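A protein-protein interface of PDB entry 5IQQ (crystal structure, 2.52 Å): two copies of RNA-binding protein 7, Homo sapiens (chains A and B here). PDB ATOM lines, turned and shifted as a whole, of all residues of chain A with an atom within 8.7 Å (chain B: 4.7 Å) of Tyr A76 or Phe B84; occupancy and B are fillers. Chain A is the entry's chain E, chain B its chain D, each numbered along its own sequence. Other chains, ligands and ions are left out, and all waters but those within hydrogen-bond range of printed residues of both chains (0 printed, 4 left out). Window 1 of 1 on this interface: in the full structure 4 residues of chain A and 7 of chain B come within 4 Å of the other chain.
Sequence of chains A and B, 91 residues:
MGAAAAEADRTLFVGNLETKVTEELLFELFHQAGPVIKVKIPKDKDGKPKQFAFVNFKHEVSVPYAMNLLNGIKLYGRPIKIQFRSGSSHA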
ATOM      1  N   ASN A  16      -3.288   7.171  15.680  1.00  0.00           N
ATOM      2  CA  ASN A  16      -3.655   7.246  17.095  1.00  0.00           C
ATOM      3  C   ASN A  16      -4.649   6.150  17.471  1.00  0.00           C
ATOM      4  O   ASN A  16      -5.625   6.390  18.184  1.00  0.00           O
ATOM      5  CB  ASN A  16      -4.220   8.625  17.442  1.00  0.00           C
ATOM      6  CG  ASN A  16      -4.153   8.926  18.927  1.00  0.00           C
ATOM      7  OD1 ASN A  16      -3.266   8.443  19.631  1.00  0.00           O
ATOM      8  ND2 ASN A  16      -5.094   9.727  19.412  1.00  0.00           N
ATOM      9  N   LEU A  17      -4.393   4.933  17.002  1.00  0.00           N
ATOM     10  CA  LEU A  17      -5.279   3.806  17.259  1.00  0.00           C
ATOM     11  C   LEU A  17      -4.918   3.134  18.575  1.00  0.00           C
ATOM     12  O   LEU A  17      -3.746   2.847  18.834  1.00  0.00           O
ATOM     13  CB  LEU A  17      -5.199   2.786  16.119  1.00  0.00           C
ATOM     14  CG  LEU A  17      -5.788   3.189  14.766  1.00  0.00           C
ATOM     15  CD1 LEU A  17      -5.592   2.072  13.756  1.00  0.00           C
ATOM     16  CD2 LEU A  17      -7.260   3.529  14.900  1.00  0.00           C
ATOM     17  N   GLU A  18      -5.925   2.882  19.405  1.00  0.00           N
ATOM     18  CA  GLU A  18      -5.717   2.037  20.570  1.00  0.00           C
ATOM     19  C   GLU A  18      -5.219   0.667  20.120  1.00  0.00           C
ATOM     20  O   GLU A  18      -5.490   0.219  19.003  1.00  0.00           O
ATOM     21  CB  GLU A  18      -7.013   1.898  21.371  1.00  0.00           C
ATOM     22  CG  GLU A  18      -6.879   1.112  22.673  1.00  0.00           C
ATOM     23  CD  GLU A  18      -6.085   1.857  23.725  1.00  0.00           C
ATOM     24  OE1 GLU A  18      -5.260   1.220  24.412  1.00  0.00           O
ATOM     25  OE2 GLU A  18      -6.288   3.081  23.864  1.00  0.00           O
ATOM     26  N   THR A  19      -4.472   0.002  21.001  1.00  0.00           N
ATOM     27  CA  THR A  19      -3.902  -1.298  20.664  1.00  0.00           C
ATOM     28  C   THR A  19      -4.972  -2.319  20.294  1.00  0.00           C
ATOM     29  O   THR A  19      -4.687  -3.252  19.537  1.00  0.00           O
ATOM     30  CB  THR A  19      -3.056  -1.810  21.836  1.00  0.00           C
ATOM     31  OG1 THR A  19      -1.870  -1.014  21.946  1.00  0.00           O
ATOM     32  CG2 THR A  19      -2.661  -3.278  21.656  1.00  0.00           C
ATOM     33  N   LYS A  20      -6.193  -2.160  20.793  1.00  0.00           N
ATOM     34  CA  LYS A  20      -7.242  -3.152  20.601  1.00  0.00           C
ATOM     35  C   LYS A  20      -8.086  -2.905  19.358  1.00  0.00           C
ATOM     36  O   LYS A  20      -9.032  -3.658  19.111  1.00  0.00           O
ATOM     37  CB  LYS A  20      -8.140  -3.191  21.836  1.00  0.00           C
ATOM     38  CG  LYS A  20      -7.389  -3.633  23.058  1.00  0.00           C
ATOM     39  CD  LYS A  20      -8.227  -3.596  24.308  1.00  0.00           C
ATOM     40  CE  LYS A  20      -7.389  -4.098  25.464  1.00  0.00           C
ATOM     41  NZ  LYS A  20      -8.118  -4.162  26.751  1.00  0.00           N
ATOM     42  N   VAL A  21      -7.769  -1.883  18.574  1.00  0.00           N
ATOM     43  CA  VAL A  21      -8.496  -1.625  17.336  1.00  0.00           C
ATOM     44  C   VAL A  21      -7.998  -2.587  16.269  1.00  0.00           C
ATOM     45  O   VAL A  21      -6.790  -2.699  16.027  1.00  0.00           O
ATOM     46  CB  VAL A  21      -8.325  -0.163  16.894  1.00  0.00           C
ATOM     47  CG1 VAL A  21      -9.003   0.067  15.546  1.00  0.00           C
ATOM     48  CG2 VAL A  21      -8.896   0.773  17.945  1.00  0.00           C
ATOM     49  N   THR A  22      -8.927  -3.287  15.630  1.00  0.00           N
ATOM     50  CA  THR A  22      -8.601  -4.254  14.597  1.00  0.00           C
ATOM     51  C   THR A  22      -9.093  -3.753  13.244  1.00  0.00           C
ATOM     52  O   THR A  22      -9.893  -2.816  13.153  1.00  0.00           O
ATOM     53  CB  THR A  22      -9.213  -5.624  14.919  1.00  0.00           C
ATOM     54  OG1 THR A  22      -8.718  -6.603  13.998  1.00  0.00           O
ATOM     55  CG2 THR A  22     -10.726  -5.585  14.822  1.00  0.00           C
ATOM     56  N   LEU A  25     -12.885  -3.890  12.916  1.00  0.00           N
ATOM     57  CA  LEU A  25     -13.627  -2.791  13.523  1.00  0.00           C
ATOM     58  C   LEU A  25     -13.605  -1.563  12.624  1.00  0.00           C
ATOM     59  O   LEU A  25     -14.641  -0.938  12.378  1.00  0.00           O
ATOM     60  CB  LEU A  25     -13.035  -2.465  14.896  1.00  0.00           C
ATOM     61  CG  LEU A  25     -13.587  -1.234  15.615  1.00  0.00           C
ATOM     62  CD1 LEU A  25     -15.062  -1.407  15.921  1.00  0.00           C
ATOM     63  CD2 LEU A  25     -12.805  -0.963  16.890  1.00  0.00           C
ATOM     64  N   LEU A  26     -12.422  -1.204  12.122  1.00  0.00           N
ATOM     65  CA  LEU A  26     -12.305  -0.020  11.281  1.00  0.00           C
ATOM     66  C   LEU A  26     -13.128  -0.170  10.010  1.00  0.00           C
ATOM     67  O   LEU A  26     -13.838   0.760   9.607  1.00  0.00           O
ATOM     68  CB  LEU A  26     -10.836   0.237  10.949  1.00  0.00           C
ATOM     69  CG  LEU A  26      -9.950   0.610  12.139  1.00  0.00           C
ATOM     70  CD1 LEU A  26      -8.502   0.761  11.700  1.00  0.00           C
ATOM     71  CD2 LEU A  26     -10.440   1.889  12.809  1.00  0.00           C
ATOM     72  N   ILE A  73     -13.274  10.546  16.640  1.00  0.00           N
ATOM     73  CA  ILE A  73     -14.144   9.658  17.403  1.00  0.00           C
ATOM     74  C   ILE A  73     -13.281   8.739  18.256  1.00  0.00           C
ATOM     75  O   ILE A  73     -12.219   8.278  17.822  1.00  0.00           O
ATOM     76  CB  ILE A  73     -15.068   8.863  16.462  1.00  0.00           C
ATOM     77  CG1 ILE A  73     -16.212   8.217  17.245  1.00  0.00           C
ATOM     78  CG2 ILE A  73     -14.289   7.795  15.707  1.00  0.00           C
ATOM     79  CD1 ILE A  73     -17.320   7.656  16.358  1.00  0.00           C
ATOM     80  N   LYS A  74     -13.730   8.475  19.480  1.00  0.00           N
ATOM     81  CA  LYS A  74     -12.938   7.731  20.451  1.00  0.00           C
ATOM     82  C   LYS A  74     -13.204   6.236  20.313  1.00  0.00           C
ATOM     83  O   LYS A  74     -14.347   5.785  20.454  1.00  0.00           O
ATOM     84  CB  LYS A  74     -13.253   8.202  21.870  1.00  0.00           C
ATOM     85  CG  LYS A  74     -12.741   9.600  22.188  1.00  0.00           C
ATOM     86  CD  LYS A  74     -13.405  10.177  23.430  1.00  0.00           C
ATOM     87  CE  LYS A  74     -13.009   9.440  24.705  1.00  0.00           C
ATOM     88  NZ  LYS A  74     -11.683   9.872  25.233  1.00  0.00           N
ATOM     89  N   LEU A  75     -12.148   5.475  20.036  1.00  0.00           N
ATOM     90  CA  LEU A  75     -12.186   4.018  20.059  1.00  0.00           C
ATOM     91  C   LEU A  75     -11.405   3.546  21.275  1.00  0.00           C
ATOM     92  O   LEU A  75     -10.205   3.815  21.387  1.00  0.00           O
ATOM     93  CB  LEU A  75     -11.594   3.422  18.783  1.00  0.00           C
ATOM     94  CG  LEU A  75     -12.246   3.843  17.468  1.00  0.00           C
ATOM     95  CD1 LEU A  75     -11.534   3.173  16.304  1.00  0.00           C
ATOM     96  CD2 LEU A  75     -13.729   3.501  17.464  1.00  0.00           C
ATOM     97  N   TYR A  76     -12.083   2.841  22.179  1.00  0.00           N
ATOM     98  CA  TYR A  76     -11.471   2.421  23.435  1.00  0.00           C
ATOM     99  C   TYR A  76     -10.837   3.617  24.142  1.00  0.00           C
ATOM    100  O   TYR A  76      -9.711   3.552  24.639  1.00  0.00           O
ATOM    101  CB  TYR A  76     -10.440   1.317  23.199  1.00  0.00           C
ATOM    102  CG  TYR A  76     -11.002   0.073  22.550  1.00  0.00           C
ATOM    103  CD1 TYR A  76     -11.613  -0.915  23.311  1.00  0.00           C
ATOM    104  CD2 TYR A  76     -10.911  -0.120  21.177  1.00  0.00           C
ATOM    105  CE1 TYR A  76     -12.124  -2.056  22.722  1.00  0.00           C
ATOM    106  CE2 TYR A  76     -11.421  -1.258  20.579  1.00  0.00           C
ATOM    107  CZ  TYR A  76     -12.025  -2.224  21.356  1.00  0.00           C
ATOM    108  OH  TYR A  76     -12.534  -3.362  20.771  1.00  0.00           O
ATOM    109  N   GLY A  77     -11.564   4.732  24.161  1.00  0.00           N
ATOM    110  CA  GLY A  77     -11.130   5.919  24.862  1.00  0.00           C
ATOM    111  C   GLY A  77     -10.107   6.772  24.144  1.00  0.00           C
ATOM    112  O   GLY A  77      -9.693   7.798  24.696  1.00  0.00           O
ATOM    113  N   ARG A  78      -9.688   6.396  22.937  1.00  0.00           N
ATOM    114  CA  ARG A  78      -8.638   7.120  22.227  1.00  0.00           C
ATOM    115  C   ARG A  78      -9.193   7.705  20.934  1.00  0.00           C
ATOM    116  O   ARG A  78      -9.686   6.947  20.080  1.00  0.00           O
ATOM    117  CB  ARG A  78      -7.450   6.204  21.926  1.00  0.00           C
ATOM    118  CG  ARG A  78      -6.260   6.939  21.334  1.00  0.00           C
ATOM    119  CD  ARG A  78      -5.068   6.024  21.133  1.00  0.00           C
ATOM    120  NE  ARG A  78      -4.731   5.288  22.348  1.00  0.00           N
ATOM    121  CZ  ARG A  78      -4.164   5.827  23.422  1.00  0.00           C
ATOM    122  NH1 ARG A  78      -3.870   7.120  23.450  1.00  0.00           N
ATOM    123  NH2 ARG A  78      -3.894   5.068  24.477  1.00  0.00           N
ATOM    124  N   PRO A  79      -9.128   9.023  20.729  1.00  0.00           N
ATOM    125  CA  PRO A  79      -9.694   9.605  19.505  1.00  0.00           C
ATOM    126  C   PRO A  79      -8.811   9.318  18.300  1.00  0.00           C
ATOM    127  O   PRO A  79      -7.606   9.580  18.318  1.00  0.00           O
ATOM    128  CB  PRO A  79      -9.746  11.103  19.819  1.00  0.00           C
ATOM    129  CG  PRO A  79      -8.598  11.308  20.744  1.00  0.00           C
ATOM    130  CD  PRO A  79      -8.491  10.049  21.574  1.00  0.00           C
ATOM    131  N   ILE A  80      -9.423   8.778  17.246  1.00  0.00           N
ATOM    132  CA  ILE A  80      -8.690   8.526  16.015  1.00  0.00           C
ATOM    133  C   ILE A  80      -8.360   9.850  15.336  1.00  0.00           C
ATOM    134  O   ILE A  80      -9.068  10.855  15.492  1.00  0.00           O
ATOM    135  CB  ILE A  80      -9.493   7.601  15.080  1.00  0.00           C
ATOM    136  CG1 ILE A  80     -10.835   8.236  14.706  1.00  0.00           C
ATOM    137  CG2 ILE A  80      -9.711   6.256  15.754  1.00  0.00           C
ATOM    138  CD1 ILE A  80     -11.592   7.475  13.629  1.00  0.00           C
ATOM    139  N   LEU B  12     -16.898  -4.633  30.545  1.00  0.00           N
ATOM    140  CA  LEU B  12     -16.585  -3.251  30.870  1.00  0.00           C
ATOM    141  C   LEU B  12     -16.677  -3.027  32.373  1.00  0.00           C
ATOM    142  O   LEU B  12     -17.507  -3.629  33.060  1.00  0.00           O
ATOM    143  CB  LEU B  12     -17.529  -2.283  30.151  1.00  0.00           C
ATOM    144  CG  LEU B  12     -17.252  -2.048  28.668  1.00  0.00           C
ATOM    145  CD1 LEU B  12     -18.380  -1.251  28.035  1.00  0.00           C
ATOM    146  CD2 LEU B  12     -15.926  -1.324  28.498  1.00  0.00           C
ATOM    147  N   GLU B  60     -17.806  -8.713  21.462  1.00  0.00           N
ATOM    148  CA  GLU B  60     -16.750  -7.786  21.850  1.00  0.00           C
ATOM    149  C   GLU B  60     -17.008  -6.387  21.299  1.00  0.00           C
ATOM    150  O   GLU B  60     -16.683  -5.386  21.948  1.00  0.00           O
ATOM    151  CB  GLU B  60     -15.399  -8.319  21.371  1.00  0.00           C
ATOM    152  CG  GLU B  60     -14.195  -7.595  21.955  1.00  0.00           C
ATOM    153  CD  GLU B  60     -13.861  -6.314  21.216  1.00  0.00           C
ATOM    154  OE1 GLU B  60     -13.985  -6.295  19.972  1.00  0.00           O
ATOM    155  OE2 GLU B  60     -13.479  -5.324  21.878  1.00  0.00           O
ATOM    156  N   VAL B  63     -18.214  -3.501  23.331  1.00  0.00           N
ATOM    157  CA  VAL B  63     -17.322  -2.820  24.265  1.00  0.00           C
ATOM    158  C   VAL B  63     -17.020  -1.420  23.736  1.00  0.00           C
ATOM    159  O   VAL B  63     -17.473  -0.435  24.335  1.00  0.00           O
ATOM    160  CB  VAL B  63     -16.044  -3.641  24.507  1.00  0.00           C
ATOM    161  CG1 VAL B  63     -15.016  -2.834  25.284  1.00  0.00           C
ATOM    162  CG2 VAL B  63     -16.377  -4.911  25.268  1.00  0.00           C
ATOM    163  N   PRO B  64     -16.285  -1.268  22.628  1.00  0.00           N
ATOM    164  CA  PRO B  64     -15.985   0.094  22.157  1.00  0.00           C
ATOM    165  C   PRO B  64     -17.234   0.894  21.840  1.00  0.00           C
ATOM    166  O   PRO B  64     -17.223   2.127  21.957  1.00  0.00           O
ATOM    167  CB  PRO B  64     -15.131  -0.149  20.906  1.00  0.00           C
ATOM    168  CG  PRO B  64     -15.561  -1.482  20.418  1.00  0.00           C
ATOM    169  CD  PRO B  64     -15.849  -2.286  21.655  1.00  0.00           C
ATOM    170  N   MET B  67     -18.947   1.970  25.484  1.00  0.00           N
ATOM    171  CA  MET B  67     -18.213   2.977  26.241  1.00  0.00           C
ATOM    172  C   MET B  67     -18.123   4.301  25.497  1.00  0.00           C
ATOM    173  O   MET B  67     -17.943   5.344  26.132  1.00  0.00           O
ATOM    174  CB  MET B  67     -16.815   2.461  26.604  1.00  0.00           C
ATOM    175  CG  MET B  67     -15.750   2.592  25.536  1.00  0.00           C
ATOM    176  SD  MET B  67     -14.169   1.923  26.110  1.00  0.00           S
ATOM    177  CE  MET B  67     -13.720   3.112  27.377  1.00  0.00           C
ATOM    178  N   ILE B  82     -16.638   4.664  32.568  1.00  0.00           N
ATOM    179  CA  ILE B  82     -16.417   3.373  31.931  1.00  0.00           C
ATOM    180  C   ILE B  82     -14.927   3.177  31.700  1.00  0.00           C
ATOM    181  O   ILE B  82     -14.205   4.116  31.343  1.00  0.00           O
ATOM    182  CB  ILE B  82     -17.203   3.265  30.611  1.00  0.00           C
ATOM    183  CG1 ILE B  82     -18.704   3.399  30.878  1.00  0.00           C
ATOM    184  CG2 ILE B  82     -16.908   1.929  29.929  1.00  0.00           C
ATOM    185  CD1 ILE B  82     -19.561   3.420  29.624  1.00  0.00           C
ATOM    186  N   GLN B  83     -14.466   1.948  31.911  1.00  0.00           N
ATOM    187  CA  GLN B  83     -13.089   1.567  31.638  1.00  0.00           C
ATOM    188  C   GLN B  83     -13.087   0.173  31.033  1.00  0.00           C
ATOM    189  O   GLN B  83     -13.835  -0.702  31.476  1.00  0.00           O
ATOM    190  CB  GLN B  83     -12.235   1.592  32.911  1.00  0.00           C
ATOM    191  CG  GLN B  83     -11.937   2.991  33.430  1.00  0.00           C
ATOM    192  CD  GLN B  83     -11.982   3.071  34.940  1.00  0.00           C
ATOM    193  OE1 GLN B  83     -12.951   3.565  35.518  1.00  0.00           O
ATOM    194  NE2 GLN B  83     -10.932   2.581  35.590  1.00  0.00           N
ATOM    195  N   PHE B  84     -12.252  -0.023  30.015  1.00  0.00           N
ATOM    196  CA  PHE B  84     -12.154  -1.298  29.320  1.00  0.00           C
ATOM    197  C   PHE B  84     -10.914  -2.037  29.801  1.00  0.00           C
ATOM    198  O   PHE B  84      -9.836  -1.443  29.917  1.00  0.00           O
ATOM    199  CB  PHE B  84     -12.099  -1.094  27.805  1.00  0.00           C
ATOM    200  CG  PHE B  84     -10.821  -0.473  27.324  1.00  0.00           C
ATOM    201  CD1 PHE B  84     -10.668   0.904  27.287  1.00  0.00           C
ATOM    202  CD2 PHE B  84      -9.770  -1.268  26.905  1.00  0.00           C
ATOM    203  CE1 PHE B  84      -9.487   1.469  26.847  1.00  0.00           C
ATOM    204  CE2 PHE B  84      -8.586  -0.709  26.463  1.00  0.00           C
ATOM    205  CZ  PHE B  84      -8.445   0.661  26.433  1.00  0.00           C
ATOM    206  N   ARG B  85     -11.071  -3.325  30.087  1.00  0.00           N
ATOM    207  CA  ARG B  85      -9.962  -4.140  30.566  1.00  0.00           C
ATOM    208  C   ARG B  85      -9.291  -4.876  29.413  1.00  0.00           C
ATOM    209  O   ARG B  85      -9.682  -5.990  29.064  1.00  0.00           O
ATOM    210  CB  ARG B  85     -10.449  -5.142  31.609  1.00  0.00           C
ATOM    211  CG  ARG B  85     -11.126  -4.502  32.813  1.00  0.00           C
ATOM    212  CD  ARG B  85     -12.583  -4.922  32.934  1.00  0.00           C
ATOM    213  NE  ARG B  85     -12.747  -6.370  32.843  1.00  0.00           N
ATOM    214  CZ  ARG B  85     -12.367  -7.231  33.782  1.00  0.00           C
ATOM    215  NH1 ARG B  85     -11.790  -6.799  34.896  1.00  0.00           N
ATOM    216  NH2 ARG B  85     -12.559  -8.532  33.605  1.00  0.00           N
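Among the printed residues, merely in contact across the chains: Glu A18 with Phe B84 (3.8 Å), Lys A20 with Phe B84 (3.3 Å), Tyr A76 with Val B63 (3.9 Å), Tyr A76 with Pro B64 (3.6 Å), Tyr A76 with Met B67 (3.8 Å) and Tyr A76 with Phe B84 (3.0 Å).
Printed residues of chain A within 4 Å of Glu B60: Tyr A76.
Of the printed residues of chain B, Glu A18 touches Phe B84.
Leu A26 touches none of the printed residues of chain B.
Among the printed residues, 8 pairs touch across the chains.
Among the printed residues, no Asp or Glu carboxylate lies within 4 Å of a Lys or Arg side-chain nitrogen of the other chain.
No position is printed for both chains.
The side-chain carboxylate (OE2) of Glu A18 is in salt-bridge range of the guanidinium group (NE) of Arg A78 (3.1 Å).
O of Arg B85 sits close to NZ of Lys A20, 3.3 Å away.
OH of Tyr A76 is in hydrogen-bond range of OE2 of Glu B60 (2.4 Å).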
